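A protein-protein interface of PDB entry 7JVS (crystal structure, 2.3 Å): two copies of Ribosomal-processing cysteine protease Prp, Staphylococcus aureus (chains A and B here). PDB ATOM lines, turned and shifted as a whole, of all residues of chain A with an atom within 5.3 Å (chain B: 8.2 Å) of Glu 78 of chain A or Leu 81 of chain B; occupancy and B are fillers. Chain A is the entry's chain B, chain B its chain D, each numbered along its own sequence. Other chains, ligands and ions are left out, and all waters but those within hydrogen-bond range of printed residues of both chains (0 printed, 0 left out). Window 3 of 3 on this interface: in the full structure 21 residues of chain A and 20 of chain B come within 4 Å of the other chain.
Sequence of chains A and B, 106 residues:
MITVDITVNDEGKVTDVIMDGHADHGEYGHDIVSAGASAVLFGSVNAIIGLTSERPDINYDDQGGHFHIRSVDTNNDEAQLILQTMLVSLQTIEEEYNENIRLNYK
The side-chain amide oxygen of Asn 76 of chain A is in hydrogen-bond range of the backbone NH of Glu 78 of chain A (3.0 Å).
N of Glu 78 of chain B sits at hydrogen-bond distance from OD1 of Asn 76 of chain B.
O of Leu 81 of chain B sits at hydrogen-bond distance from OG1 of Thr 85 of chain B.
Among the printed residues, merely in contact across the chains: Ile 82 of chain A with Thr 85 of chain B, Leu 81 of chain A with Glu 78 of chain B, Leu 51 of chain A with Gln 84 of chain B, Leu 51 of chain A with Thr 85 of chain B and Glu 78 of chain A with Leu 81 of chain B.
Asn 76 of chain A touches none of the printed residues of chain B.
Glu 78 of chain A touches just one residue of chain B: Leu 81 (3.8 Å).
No residue of chain B comes within 4 Å of Ala 79 of chain A.
Of the printed residues of chain B, Leu 81 of chain A touches Glu 78 (3.7 Å).
Of chain A, only Glu 78 (3.8 Å) comes within 4 Å of Leu 81 of chain B.
Ile 82 of chain B touches none of the printed residues of chain A.
Printed residues of chain A within 4 Å of Gln 84 of chain B: Leu 51 (3.8 Å).
Of the printed residues of chain A, Thr 85 of chain B touches Leu 51 and Ile 82.
The nearest printed residue of chain B that does not touch Glu 78 of chain A is Thr 85 of chain B (6.5 Å).
The nearest residue of chain A that does not touch Leu 81 of chain B is Leu 81 of chain A (4.1 Å).
The nearest printed residue of chain A that does not touch Glu 78 of chain B is Asp 77 of chain A (6.6 Å).
Printed residues of chain A that touch a printed residue of chain B: Leu 51, Glu 78, Leu 81 and Ile 82.
Of the 18 printed residues of chain B, 4 touch a printed residue of chain A.
Glu 78 of chain A touches Leu 81 of chain B, and with the chains exchanged Leu 81 of chain A touches Glu 78 of chain B.
8 positions are printed for both chains.
Of the 5 pairs that touch across the chains among the printed residues, 2 have their exchanged pair printed and touching as well.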
ATOM      1  N   LEU A  51      24.847  -3.605 -25.971  1.00  0.00           N
ATOM      2  CA  LEU A  51      24.154  -3.723 -24.682  1.00  0.00           C
ATOM      3  C   LEU A  51      25.073  -3.842 -23.469  1.00  0.00           C
ATOM      4  O   LEU A  51      24.614  -3.705 -22.336  1.00  0.00           O
ATOM      5  CB  LEU A  51      23.200  -4.916 -24.711  1.00  0.00           C
ATOM      6  CG  LEU A  51      22.179  -4.927 -25.848  1.00  0.00           C
ATOM      7  CD1 LEU A  51      21.369  -6.221 -25.816  1.00  0.00           C
ATOM      8  CD2 LEU A  51      21.277  -3.696 -25.750  1.00  0.00           C
ATOM      9  N   THR A  52      26.359  -4.097 -23.706  1.00  0.00           N
ATOM     10  CA  THR A  52      27.332  -4.273 -22.641  1.00  0.00           C
ATOM     11  C   THR A  52      28.577  -3.411 -22.886  1.00  0.00           C
ATOM     12  O   THR A  52      28.743  -2.791 -23.940  1.00  0.00           O
ATOM     13  CB  THR A  52      27.779  -5.746 -22.534  1.00  0.00           C
ATOM     14  OG1 THR A  52      28.790  -6.024 -23.519  1.00  0.00           O
ATOM     15  CG2 THR A  52      26.591  -6.678 -22.727  1.00  0.00           C
ATOM     16  N   SER A  53      29.467  -3.411 -21.891  1.00  0.00           N
ATOM     17  CA  SER A  53      30.717  -2.674 -21.937  1.00  0.00           C
ATOM     18  C   SER A  53      31.882  -3.479 -22.519  1.00  0.00           C
ATOM     19  O   SER A  53      33.001  -2.972 -22.611  1.00  0.00           O
ATOM     20  CB  SER A  53      31.051  -2.189 -20.525  1.00  0.00           C
ATOM     21  OG  SER A  53      30.972  -3.244 -19.592  1.00  0.00           O
ATOM     22  N   ASN A  76      32.853 -10.339 -17.737  1.00  0.00           N
ATOM     23  CA  ASN A  76      31.644  -9.576 -18.020  1.00  0.00           C
ATOM     24  C   ASN A  76      30.447 -10.545 -18.041  1.00  0.00           C
ATOM     25  O   ASN A  76      30.363 -11.393 -18.929  1.00  0.00           O
ATOM     26  CB  ASN A  76      31.779  -8.853 -19.358  1.00  0.00           C
ATOM     27  CG  ASN A  76      30.638  -7.891 -19.621  1.00  0.00           C
ATOM     28  OD1 ASN A  76      29.467  -8.252 -19.505  1.00  0.00           O
ATOM     29  ND2 ASN A  76      30.975  -6.658 -19.978  1.00  0.00           N
ATOM     30  N   ASP A  77      29.528 -10.432 -17.079  1.00  0.00           N
ATOM     31  CA  ASP A  77      28.433 -11.321 -17.005  1.00  0.00           C
ATOM     32  C   ASP A  77      27.427 -11.079 -18.066  1.00  0.00           C
ATOM     33  O   ASP A  77      26.892 -11.984 -18.548  1.00  0.00           O
ATOM     34  CB  ASP A  77      27.792 -11.211 -15.652  1.00  0.00           C
ATOM     35  CG  ASP A  77      28.631 -11.804 -14.567  1.00  0.00           C
ATOM     36  OD1 ASP A  77      29.564 -12.535 -14.840  1.00  0.00           O
ATOM     37  OD2 ASP A  77      28.364 -11.529 -13.433  1.00  0.00           O
ATOM     38  N   GLU A  78      27.159  -9.860 -18.431  1.00  0.00           N
ATOM     39  CA  GLU A  78      26.219  -9.615 -19.474  1.00  0.00           C
ATOM     40  C   GLU A  78      26.708 -10.203 -20.783  1.00  0.00           C
ATOM     41  O   GLU A  78      25.987 -10.822 -21.463  1.00  0.00           O
ATOM     42  CB  GLU A  78      25.964  -8.148 -19.635  1.00  0.00           C
ATOM     43  CG  GLU A  78      25.200  -7.564 -18.514  1.00  0.00           C
ATOM     44  CD  GLU A  78      24.633  -6.247 -18.876  1.00  0.00           C
ATOM     45  OE1 GLU A  78      25.216  -5.565 -19.673  1.00  0.00           O
ATOM     46  OE2 GLU A  78      23.599  -5.893 -18.386  1.00  0.00           O
ATOM     47  N   ALA A  79      27.958 -10.036 -21.111  1.00  0.00           N
ATOM     48  CA  ALA A  79      28.463 -10.585 -22.332  1.00  0.00           C
ATOM     49  C   ALA A  79      28.492 -12.113 -22.379  1.00  0.00           C
ATOM     50  O   ALA A  79      28.287 -12.686 -23.424  1.00  0.00           O
ATOM     51  CB  ALA A  79      29.835 -10.006 -22.631  1.00  0.00           C
ATOM     52  N   GLN A  80      28.711 -12.750 -21.244  1.00  0.00           N
ATOM     53  CA  GLN A  80      28.781 -14.178 -21.174  1.00  0.00           C
ATOM     54  C   GLN A  80      27.431 -14.827 -21.309  1.00  0.00           C
ATOM     55  O   GLN A  80      27.321 -15.913 -21.771  1.00  0.00           O
ATOM     56  CB  GLN A  80      29.422 -14.613 -19.876  1.00  0.00           C
ATOM     57  CG  GLN A  80      30.919 -14.484 -19.868  1.00  0.00           C
ATOM     58  CD  GLN A  80      31.659 -15.484 -20.707  1.00  0.00           C
ATOM     59  OE1 GLN A  80      31.424 -16.630 -20.653  1.00  0.00           O
ATOM     60  NE2 GLN A  80      32.582 -15.019 -21.457  1.00  0.00           N
ATOM     61  N   LEU A  81      26.414 -14.142 -20.888  1.00  0.00           N
ATOM     62  CA  LEU A  81      25.046 -14.610 -21.028  1.00  0.00           C
ATOM     63  C   LEU A  81      24.586 -14.550 -22.501  1.00  0.00           C
ATOM     64  O   LEU A  81      23.822 -15.420 -22.967  1.00  0.00           O
ATOM     65  CB  LEU A  81      24.106 -13.789 -20.130  1.00  0.00           C
ATOM     66  CG  LEU A  81      22.637 -14.229 -20.143  1.00  0.00           C
ATOM     67  CD1 LEU A  81      22.515 -15.660 -19.638  1.00  0.00           C
ATOM     68  CD2 LEU A  81      21.758 -13.303 -19.326  1.00  0.00           C
ATOM     69  N   ILE A  82      25.043 -13.514 -23.216  1.00  0.00           N
ATOM     70  CA  ILE A  82      24.732 -13.352 -24.637  1.00  0.00           C
ATOM     71  C   ILE A  82      25.418 -14.456 -25.438  1.00  0.00           C
ATOM     72  O   ILE A  82      24.820 -15.027 -26.337  1.00  0.00           O
ATOM     73  CB  ILE A  82      25.124 -11.963 -25.185  1.00  0.00           C
ATOM     74  CG1 ILE A  82      24.293 -10.886 -24.511  1.00  0.00           C
ATOM     75  CG2 ILE A  82      24.906 -11.902 -26.686  1.00  0.00           C
ATOM     76  CD1 ILE A  82      24.775  -9.480 -24.786  1.00  0.00           C
ATOM     77  N   LYS B  13      10.624  -2.469 -19.490  1.00  0.00           N
ATOM     78  CA  LYS B  13      10.714  -3.907 -19.542  1.00  0.00           C
ATOM     79  C   LYS B  13       9.893  -4.476 -20.711  1.00  0.00           C
ATOM     80  O   LYS B  13       8.726  -4.125 -20.881  1.00  0.00           O
ATOM     81  CB  LYS B  13      10.215  -4.509 -18.227  1.00  0.00           C
ATOM     82  CG  LYS B  13      10.987  -4.048 -16.998  1.00  0.00           C
ATOM     83  CD  LYS B  13      12.449  -3.781 -17.319  1.00  0.00           C
ATOM     84  CE  LYS B  13      13.355  -4.160 -16.157  1.00  0.00           C
ATOM     85  NZ  LYS B  13      12.681  -4.002 -14.838  1.00  0.00           N
ATOM     86  N   VAL B  14      10.503  -5.348 -21.510  1.00  0.00           N
ATOM     87  CA  VAL B  14       9.826  -6.010 -22.622  1.00  0.00           C
ATOM     88  C   VAL B  14       8.796  -7.016 -22.094  1.00  0.00           C
ATOM     89  O   VAL B  14       9.146  -7.949 -21.358  1.00  0.00           O
ATOM     90  CB  VAL B  14      10.828  -6.732 -23.543  1.00  0.00           C
ATOM     91  CG1 VAL B  14      10.108  -7.417 -24.696  1.00  0.00           C
ATOM     92  CG2 VAL B  14      11.854  -5.749 -24.070  1.00  0.00           C
ATOM     93  N   SER B  44      16.133 -17.696 -28.670  1.00  0.00           N
ATOM     94  CA  SER B  44      16.040 -16.834 -27.501  1.00  0.00           C
ATOM     95  C   SER B  44      15.156 -17.441 -26.420  1.00  0.00           C
ATOM     96  O   SER B  44      15.521 -17.455 -25.266  1.00  0.00           O
ATOM     97  CB  SER B  44      15.481 -15.463 -27.895  1.00  0.00           C
ATOM     98  OG  SER B  44      16.338 -14.862 -28.833  1.00  0.00           O
ATOM     99  N   ILE B  48      16.043 -18.530 -22.692  1.00  0.00           N
ATOM    100  CA  ILE B  48      15.342 -17.965 -21.547  1.00  0.00           C
ATOM    101  C   ILE B  48      14.808 -19.067 -20.636  1.00  0.00           C
ATOM    102  O   ILE B  48      14.616 -18.854 -19.438  1.00  0.00           O
ATOM    103  CB  ILE B  48      14.163 -17.083 -21.994  1.00  0.00           C
ATOM    104  CG1 ILE B  48      14.674 -15.742 -22.521  1.00  0.00           C
ATOM    105  CG2 ILE B  48      13.196 -16.863 -20.841  1.00  0.00           C
ATOM    106  CD1 ILE B  48      13.615 -14.916 -23.217  1.00  0.00           C
ATOM    107  N   THR B  52      17.819 -19.032 -17.404  1.00  0.00           N
ATOM    108  CA  THR B  52      17.234 -18.219 -16.392  1.00  0.00           C
ATOM    109  C   THR B  52      16.123 -18.950 -15.709  1.00  0.00           C
ATOM    110  O   THR B  52      15.803 -20.012 -16.049  1.00  0.00           O
ATOM    111  CB  THR B  52      16.651 -16.931 -16.968  1.00  0.00           C
ATOM    112  OG1 THR B  52      15.392 -17.182 -17.523  1.00  0.00           O
ATOM    113  CG2 THR B  52      17.460 -16.373 -17.994  1.00  0.00           C
ATOM    114  N   ASN B  76      13.021 -10.058 -14.207  1.00  0.00           N
ATOM    115  CA  ASN B  76      14.122 -11.007 -14.320  1.00  0.00           C
ATOM    116  C   ASN B  76      15.180 -10.366 -15.211  1.00  0.00           C
ATOM    117  O   ASN B  76      15.051 -10.402 -16.435  1.00  0.00           O
ATOM    118  CB  ASN B  76      13.641 -12.323 -14.927  1.00  0.00           C
ATOM    119  CG  ASN B  76      14.706 -13.400 -14.900  1.00  0.00           C
ATOM    120  OD1 ASN B  76      15.828 -13.192 -15.362  1.00  0.00           O
ATOM    121  ND2 ASN B  76      14.359 -14.562 -14.358  1.00  0.00           N
ATOM    122  N   ASP B  77      16.218  -9.773 -14.620  1.00  0.00           N
ATOM    123  CA  ASP B  77      17.212  -9.113 -15.413  1.00  0.00           C
ATOM    124  C   ASP B  77      17.853  -9.960 -16.496  1.00  0.00           C
ATOM    125  O   ASP B  77      18.171  -9.425 -17.512  1.00  0.00           O
ATOM    126  CB  ASP B  77      18.300  -8.527 -14.521  1.00  0.00           C
ATOM    127  CG  ASP B  77      17.780  -7.561 -13.482  1.00  0.00           C
ATOM    128  OD1 ASP B  77      16.939  -6.705 -13.734  1.00  0.00           O
ATOM    129  OD2 ASP B  77      18.237  -7.660 -12.358  1.00  0.00           O
ATOM    130  N   GLU B  78      18.077 -11.243 -16.279  1.00  0.00           N
ATOM    131  CA  GLU B  78      18.710 -12.078 -17.273  1.00  0.00           C
ATOM    132  C   GLU B  78      17.781 -12.319 -18.462  1.00  0.00           C
ATOM    133  O   GLU B  78      18.182 -12.212 -19.561  1.00  0.00           O
ATOM    134  CB  GLU B  78      19.163 -13.404 -16.682  1.00  0.00           C
ATOM    135  CG  GLU B  78      20.088 -13.326 -15.494  1.00  0.00           C
ATOM    136  CD  GLU B  78      20.710 -14.651 -15.112  1.00  0.00           C
ATOM    137  OE1 GLU B  78      20.165 -15.390 -14.308  1.00  0.00           O
ATOM    138  OE2 GLU B  78      21.768 -14.977 -15.595  1.00  0.00           O
ATOM    139  N   ALA B  79      16.543 -12.692 -18.205  1.00  0.00           N
ATOM    140  CA  ALA B  79      15.552 -12.881 -19.249  1.00  0.00           C
ATOM    141  C   ALA B  79      15.417 -11.617 -20.106  1.00  0.00           C
ATOM    142  O   ALA B  79      15.355 -11.701 -21.336  1.00  0.00           O
ATOM    143  CB  ALA B  79      14.209 -13.276 -18.647  1.00  0.00           C
ATOM    144  N   GLN B  80      15.404 -10.452 -19.442  1.00  0.00           N
ATOM    145  CA  GLN B  80      15.236  -9.152 -20.093  1.00  0.00           C
ATOM    146  C   GLN B  80      16.420  -8.779 -21.005  1.00  0.00           C
ATOM    147  O   GLN B  80      16.238  -8.124 -22.036  1.00  0.00           O
ATOM    148  CB  GLN B  80      14.980  -8.054 -19.060  1.00  0.00           C
ATOM    149  CG  GLN B  80      13.547  -8.072 -18.513  1.00  0.00           C
ATOM    150  CD  GLN B  80      12.518  -7.577 -19.516  1.00  0.00           C
ATOM    151  OE1 GLN B  80      12.756  -6.606 -20.205  1.00  0.00           O
ATOM    152  NE2 GLN B  80      11.371  -8.242 -19.592  1.00  0.00           N
ATOM    153  N   LEU B  81      17.626  -9.210 -20.628  1.00  0.00           N
ATOM    154  CA  LEU B  81      18.768  -8.953 -21.494  1.00  0.00           C
ATOM    155  C   LEU B  81      18.783  -9.931 -22.686  1.00  0.00           C
ATOM    156  O   LEU B  81      19.200  -9.562 -23.816  1.00  0.00           O
ATOM    157  CB  LEU B  81      20.062  -9.045 -20.687  1.00  0.00           C
ATOM    158  CG  LEU B  81      21.383  -9.006 -21.444  1.00  0.00           C
ATOM    159  CD1 LEU B  81      21.686  -7.607 -21.964  1.00  0.00           C
ATOM    160  CD2 LEU B  81      22.494  -9.504 -20.537  1.00  0.00           C
ATOM    161  N   ILE B  82      18.223 -11.135 -22.522  1.00  0.00           N
ATOM    162  CA  ILE B  82      18.061 -12.075 -23.641  1.00  0.00           C
ATOM    163  C   ILE B  82      17.043 -11.512 -24.626  1.00  0.00           C
ATOM    164  O   ILE B  82      17.238 -11.580 -25.832  1.00  0.00           O
ATOM    165  CB  ILE B  82      17.665 -13.488 -23.186  1.00  0.00           C
ATOM    166  CG1 ILE B  82      18.812 -14.123 -22.406  1.00  0.00           C
ATOM    167  CG2 ILE B  82      17.327 -14.369 -24.385  1.00  0.00           C
ATOM    168  CD1 ILE B  82      18.426 -15.404 -21.684  1.00  0.00           C
ATOM    169  N   LEU B  83      15.968 -10.920 -24.101  1.00  0.00           N
ATOM    170  CA  LEU B  83      14.963 -10.271 -24.948  1.00  0.00           C
ATOM    171  C   LEU B  83      15.530  -9.051 -25.696  1.00  0.00           C
ATOM    172  O   LEU B  83      15.203  -8.844 -26.855  1.00  0.00           O
ATOM    173  CB  LEU B  83      13.732  -9.894 -24.142  1.00  0.00           C
ATOM    174  CG  LEU B  83      12.810 -11.036 -23.738  1.00  0.00           C
ATOM    175  CD1 LEU B  83      11.851 -10.583 -22.660  1.00  0.00           C
ATOM    176  CD2 LEU B  83      12.000 -11.583 -24.903  1.00  0.00           C
ATOM    177  N   GLN B  84      16.359  -8.269 -25.010  1.00  0.00           N
ATOM    178  CA  GLN B  84      16.869  -7.099 -25.711  1.00  0.00           C
ATOM    179  C   GLN B  84      17.959  -7.533 -26.679  1.00  0.00           C
ATOM    180  O   GLN B  84      18.119  -6.955 -27.754  1.00  0.00           O
ATOM    181  CB  GLN B  84      17.505  -6.134 -24.711  1.00  0.00           C
ATOM    182  CG  GLN B  84      16.518  -5.499 -23.746  1.00  0.00           C
ATOM    183  CD  GLN B  84      16.058  -4.125 -24.203  1.00  0.00           C
ATOM    184  OE1 GLN B  84      14.861  -3.842 -24.250  1.00  0.00           O
ATOM    185  NE2 GLN B  84      17.014  -3.264 -24.542  1.00  0.00           N
ATOM    186  N   THR B  85      18.595  -8.677 -26.448  1.00  0.00           N
ATOM    187  CA  THR B  85      19.552  -9.226 -27.396  1.00  0.00           C
ATOM    188  C   THR B  85      18.816  -9.675 -28.651  1.00  0.00           C
ATOM    189  O   THR B  85      19.311  -9.521 -29.766  1.00  0.00           O
ATOM    190  CB  THR B  85      20.309 -10.426 -26.799  1.00  0.00           C
ATOM    191  OG1 THR B  85      21.121  -9.988 -25.704  1.00  0.00           O
ATOM    192  CG2 THR B  85      21.189 -11.081 -27.852  1.00  0.00           C
ATOM    193  N   MET B  86      17.633 -10.249 -28.452  1.00  0.00           N
ATOM    194  CA  MET B  86      16.812 -10.722 -29.557  1.00  0.00           C
ATOM    195  C   MET B  86      16.392  -9.540 -30.418  1.00  0.00           C
ATOM    196  O   MET B  86      16.456  -9.596 -31.645  1.00  0.00           O
ATOM    197  CB  MET B  86      15.573 -11.445 -29.026  1.00  0.00           C
ATOM    198  CG  MET B  86      14.754 -12.142 -30.099  1.00  0.00           C
ATOM    199  SD  MET B  86      13.270 -12.925 -29.439  1.00  0.00           S
ATOM    200  CE  MET B  86      12.310 -11.487 -28.975  1.00  0.00           C
ATOM    201  N   LEU B  87      15.962  -8.466 -29.762  1.00  0.00           N
ATOM    202  CA  LEU B  87      15.539  -7.261 -30.460  1.00  0.00           C
ATOM    203  C   LEU B  87      16.671  -6.738 -31.333  1.00  0.00           C
ATOM    204  O   LEU B  87      16.465  -6.405 -32.499  1.00  0.00           O
ATOM    205  CB  LEU B  87      15.114  -6.187 -29.456  1.00  0.00           C
ATOM    206  CG  LEU B  87      13.878  -6.529 -28.623  1.00  0.00           C
ATOM    207  CD1 LEU B  87      13.631  -5.468 -27.563  1.00  0.00           C
ATOM    208  CD2 LEU B  87      12.665  -6.681 -29.525  1.00  0.00           C
ATOM    209  N   VAL B  88      17.869  -6.666 -30.759  1.00  0.00           N
ATOM    210  CA  VAL B  88      19.035  -6.191 -31.489  1.00  0.00           C
ATOM    211  C   VAL B  88      19.281  -7.053 -32.722  1.00  0.00           C
ATOM    212  O   VAL B  88      19.528  -6.533 -33.810  1.00  0.00           O
ATOM    213  CB  VAL B  88      20.300  -6.216 -30.612  1.00  0.00           C
ATOM    214  CG1 VAL B  88      21.540  -6.021 -31.471  1.00  0.00           C
ATOM    215  CG2 VAL B  88      20.217  -5.149 -29.531  1.00  0.00           C
